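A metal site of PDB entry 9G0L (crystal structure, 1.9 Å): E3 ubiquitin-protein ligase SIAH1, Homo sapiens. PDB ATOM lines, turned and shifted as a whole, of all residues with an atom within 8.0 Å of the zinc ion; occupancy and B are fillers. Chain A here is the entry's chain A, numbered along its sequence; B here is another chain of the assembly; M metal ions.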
ATOM      1  N   GLN A  28       3.559  25.471  12.229  1.00  0.00           N
ATOM      2  CA  GLN A  28       3.537  24.439  13.263  1.00  0.00           C
ATOM      3  C   GLN A  28       2.498  23.371  12.963  1.00  0.00           C
ATOM      4  O   GLN A  28       1.557  23.592  12.202  1.00  0.00           O
ATOM      5  CB  GLN A  28       3.238  25.024  14.636  1.00  0.00           C
ATOM      6  CG  GLN A  28       1.818  25.544  14.733  1.00  0.00           C
ATOM      7  CD  GLN A  28       1.404  25.878  16.155  1.00  0.00           C
ATOM      8  OE1 GLN A  28       2.021  26.710  16.842  1.00  0.00           O
ATOM      9  NE2 GLN A  28       0.371  25.195  16.620  1.00  0.00           N
ATOM     10  N   CYS A  29       2.648  22.212  13.594  1.00  0.00           N
ATOM     11  CA  CYS A  29       1.650  21.158  13.496  1.00  0.00           C
ATOM     12  C   CYS A  29       0.457  21.479  14.392  1.00  0.00           C
ATOM     13  O   CYS A  29       0.464  22.446  15.163  1.00  0.00           O
ATOM     14  CB  CYS A  29       2.239  19.809  13.887  1.00  0.00           C
ATOM     15  SG  CYS A  29       2.491  19.678  15.699  1.00  0.00           S
ATOM     16  N   GLN A  30      -0.560  20.609  14.312  1.00  0.00           N
ATOM     17  CA  GLN A  30      -1.779  20.745  15.122  1.00  0.00           C
ATOM     18  C   GLN A  30      -1.475  20.871  16.617  1.00  0.00           C
ATOM     19  O   GLN A  30      -2.211  21.550  17.335  1.00  0.00           O
ATOM     20  CB  GLN A  30      -2.687  19.539  14.877  1.00  0.00           C
ATOM     21  CG  GLN A  30      -3.908  19.457  15.798  1.00  0.00           C
ATOM     22  CD  GLN A  30      -5.045  20.325  15.290  1.00  0.00           C
ATOM     23  OE1 GLN A  30      -5.122  20.627  14.098  1.00  0.00           O
ATOM     24  NE2 GLN A  30      -5.919  20.746  16.200  1.00  0.00           N
ATOM     25  N   SER A  31      -0.453  20.174  17.119  1.00  0.00           N
ATOM     26  CA  SER A  31      -0.154  20.131  18.553  1.00  0.00           C
ATOM     27  C   SER A  31       0.932  21.122  18.992  1.00  0.00           C
ATOM     28  O   SER A  31       1.349  21.085  20.164  1.00  0.00           O
ATOM     29  CB  SER A  31       0.206  18.696  18.943  1.00  0.00           C
ATOM     30  OG  SER A  31      -0.826  17.787  18.539  1.00  0.00           O
ATOM     31  N   GLY A  32       1.388  22.002  18.106  1.00  0.00           N
ATOM     32  CA  GLY A  32       2.259  23.113  18.473  1.00  0.00           C
ATOM     33  C   GLY A  32       3.765  22.926  18.322  1.00  0.00           C
ATOM     34  O   GLY A  32       4.523  23.722  18.899  1.00  0.00           O
ATOM     35  N   HIS A  33       4.208  21.963  17.534  1.00  0.00           N
ATOM     36  CA  HIS A  33       5.629  21.700  17.352  1.00  0.00           C
ATOM     37  C   HIS A  33       6.145  22.431  16.124  1.00  0.00           C
ATOM     38  O   HIS A  33       5.454  22.512  15.111  1.00  0.00           O
ATOM     39  CB  HIS A  33       5.864  20.197  17.202  1.00  0.00           C
ATOM     40  CG  HIS A  33       5.245  19.394  18.308  1.00  0.00           C
ATOM     41  ND1 HIS A  33       4.398  18.332  18.087  1.00  0.00           N
ATOM     42  CD2 HIS A  33       5.301  19.563  19.653  1.00  0.00           C
ATOM     43  CE1 HIS A  33       3.999  17.848  19.252  1.00  0.00           C
ATOM     44  NE2 HIS A  33       4.532  18.591  20.214  1.00  0.00           N
ATOM     45  N   LEU A  34       7.377  22.931  16.220  1.00  0.00           N
ATOM     46  CA  LEU A  34       7.974  23.786  15.214  1.00  0.00           C
ATOM     47  C   LEU A  34       9.022  22.990  14.426  1.00  0.00           C
ATOM     48  O   LEU A  34       9.633  22.066  14.959  1.00  0.00           O
ATOM     49  CB  LEU A  34       8.643  24.997  15.875  1.00  0.00           C
ATOM     50  CG  LEU A  34       7.861  25.963  16.793  1.00  0.00           C
ATOM     51  CD1 LEU A  34       8.654  27.246  16.940  1.00  0.00           C
ATOM     52  CD2 LEU A  34       6.498  26.297  16.272  1.00  0.00           C
ATOM     53  N   VAL A  35       9.205  23.349  13.153  1.00  0.00           N
ATOM     54  CA  VAL A  35      10.309  22.847  12.322  1.00  0.00           C
ATOM     55  C   VAL A  35      10.774  23.996  11.435  1.00  0.00           C
ATOM     56  O   VAL A  35       9.943  24.751  10.915  1.00  0.00           O
ATOM     57  CB  VAL A  35       9.914  21.665  11.407  1.00  0.00           C
ATOM     58  CG1 VAL A  35      11.149  20.904  10.964  1.00  0.00           C
ATOM     59  CG2 VAL A  35       8.924  20.759  12.082  1.00  0.00           C
ATOM     60  N   CYS A  45       6.379  14.464   7.956  1.00  0.00           N
ATOM     61  CA  CYS A  45       5.485  14.629   9.092  1.00  0.00           C
ATOM     62  C   CYS A  45       6.266  15.328  10.204  1.00  0.00           C
ATOM     63  O   CYS A  45       7.482  15.476  10.134  1.00  0.00           O
ATOM     64  CB  CYS A  45       4.930  13.281   9.570  1.00  0.00           C
ATOM     65  SG  CYS A  45       6.183  12.056   9.953  1.00  0.00           S
ATOM     66  N   CYS A  46       5.539  15.739  11.223  1.00  0.00           N
ATOM     67  CA  CYS A  46       6.124  16.457  12.324  1.00  0.00           C
ATOM     68  C   CYS A  46       7.163  15.580  13.008  1.00  0.00           C
ATOM     69  O   CYS A  46       6.827  14.456  13.399  1.00  0.00           O
ATOM     70  CB  CYS A  46       5.041  16.864  13.317  1.00  0.00           C
ATOM     71  SG  CYS A  46       5.692  17.640  14.798  1.00  0.00           S
ATOM     72  N   PRO A  47       8.411  16.020  13.137  1.00  0.00           N
ATOM     73  CA  PRO A  47       9.422  15.158  13.768  1.00  0.00           C
ATOM     74  C   PRO A  47       9.159  14.897  15.224  1.00  0.00           C
ATOM     75  O   PRO A  47       9.690  13.927  15.781  1.00  0.00           O
ATOM     76  CB  PRO A  47      10.731  15.932  13.579  1.00  0.00           C
ATOM     77  CG  PRO A  47      10.370  17.269  13.020  1.00  0.00           C
ATOM     78  CD  PRO A  47       8.880  17.403  12.985  1.00  0.00           C
ATOM     79  N   THR A  48       8.366  15.733  15.888  1.00  0.00           N
ATOM     80  CA  THR A  48       8.114  15.539  17.310  1.00  0.00           C
ATOM     81  C   THR A  48       6.956  14.582  17.542  1.00  0.00           C
ATOM     82  O   THR A  48       7.100  13.621  18.307  1.00  0.00           O
ATOM     83  CB  THR A  48       7.858  16.899  17.990  1.00  0.00           C
ATOM     84  OG1 THR A  48       8.988  17.775  17.799  1.00  0.00           O
ATOM     85  CG2 THR A  48       7.582  16.717  19.478  1.00  0.00           C
ATOM     86  N   CYS A  49       5.806  14.797  16.908  1.00  0.00           N
ATOM     87  CA  CYS A  49       4.650  13.960  17.178  1.00  0.00           C
ATOM     88  C   CYS A  49       4.266  13.017  16.040  1.00  0.00           C
ATOM     89  O   CYS A  49       3.387  12.173  16.240  1.00  0.00           O
ATOM     90  CB  CYS A  49       3.427  14.822  17.522  1.00  0.00           C
ATOM     91  SG  CYS A  49       2.776  15.753  16.161  1.00  0.00           S
ATOM     92  N   ARG A  50       4.900  13.130  14.881  1.00  0.00           N
ATOM     93  CA  ARG A  50       4.630  12.345  13.678  1.00  0.00           C
ATOM     94  C   ARG A  50       3.251  12.628  13.085  1.00  0.00           C
ATOM     95  O   ARG A  50       2.828  11.927  12.164  1.00  0.00           O
ATOM     96  CB  ARG A  50       4.793  10.838  13.934  1.00  0.00           C
ATOM     97  CG  ARG A  50       6.155  10.463  14.475  1.00  0.00           C
ATOM     98  CD  ARG A  50       6.135   9.088  15.128  1.00  0.00           C
ATOM     99  NE  ARG A  50       5.838   7.973  14.227  1.00  0.00           N
ATOM    100  CZ  ARG A  50       6.314   7.810  12.983  1.00  0.00           C
ATOM    101  NH1 ARG A  50       7.203   8.637  12.459  1.00  0.00           N
ATOM    102  NH2 ARG A  50       5.887   6.773  12.266  1.00  0.00           N
ATOM    103  N   GLY A  51       2.548  13.629  13.596  1.00  0.00           N
ATOM    104  CA  GLY A  51       1.393  14.159  12.925  1.00  0.00           C
ATOM    105  C   GLY A  51       1.782  14.875  11.633  1.00  0.00           C
ATOM    106  O   GLY A  51       2.961  15.097  11.365  1.00  0.00           O
ATOM    107  N   PRO A  52       0.807  15.229  10.817  1.00  0.00           N
ATOM    108  CA  PRO A  52       1.116  15.988   9.596  1.00  0.00           C
ATOM    109  C   PRO A  52       1.845  17.287   9.905  1.00  0.00           C
ATOM    110  O   PRO A  52       1.685  17.904  10.975  1.00  0.00           O
ATOM    111  CB  PRO A  52      -0.255  16.249   8.965  1.00  0.00           C
ATOM    112  CG  PRO A  52      -1.176  15.255   9.605  1.00  0.00           C
ATOM    113  CD  PRO A  52      -0.643  15.001  10.976  1.00  0.00           C
ATOM    114  N   LEU A  53       2.733  17.645   8.995  1.00  0.00           N
ATOM    115  CA  LEU A  53       3.474  18.894   9.131  1.00  0.00           C
ATOM    116  C   LEU A  53       2.515  20.074   9.020  1.00  0.00           C
ATOM    117  O   LEU A  53       2.502  20.964   9.873  1.00  0.00           O
ATOM    118  CB  LEU A  53       4.538  18.948   8.049  1.00  0.00           C
ATOM    119  CG  LEU A  53       5.873  18.289   8.391  1.00  0.00           C
ATOM    120  CD1 LEU A  53       6.717  18.140   7.134  1.00  0.00           C
ATOM    121  CD2 LEU A  53       6.620  19.068   9.466  1.00  0.00           C
ATOM    122  N   LEU B  59       1.843  25.843  21.799  1.00  0.00           N
ATOM    123  CA  LEU B  59       2.747  25.497  22.900  1.00  0.00           C
ATOM    124  C   LEU B  59       3.861  26.522  23.042  1.00  0.00           C
ATOM    125  O   LEU B  59       4.294  26.809  24.158  1.00  0.00           O
ATOM    126  CB  LEU B  59       3.376  24.120  22.677  1.00  0.00           C
ATOM    127  CG  LEU B  59       2.545  22.853  22.823  1.00  0.00           C
ATOM    128  CD1 LEU B  59       3.418  21.702  22.403  1.00  0.00           C
ATOM    129  CD2 LEU B  59       2.052  22.662  24.265  1.00  0.00           C
HETATM  130 ZN    ZN M   1       3.848  17.832  16.156  1.00  0.00          ZN
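The side-chain sulfur of Cys 49 sits close to the backbone NH of Gly 51 (3.3 Å). The backbone carbonyl oxygen of Gly 51 lies within hydrogen-bond range of the backbone NH of Cys 46. The backbone NH of Gly 32 sits close to the side-chain sulfur of Cys 29, at 3.5 Å. The side-chain sulfur (SG) of Cys 29 sits close to the backbone NH (N) of Ser 31. The side-chain sulfur (SG) of Cys 46 lies close to the backbone NH (N) of Thr 48, at 3.5 Å.
Four residues have an atom within 4 Å of the zinc ion: Cys 29, His 33, Cys 46 and Cys 49.
The zinc ion is bound by a ring nitrogen (ND1) of His 33 (2.1 Å), the side-chain sulfur (SG) of Cys 46 (2.3 Å), the side-chain sulfur (SG) of Cys 29 (2.3 Å) and the side-chain sulfur (SG) of Cys 49 (2.3 Å). The zinc ion has four donor atoms within binding distance.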
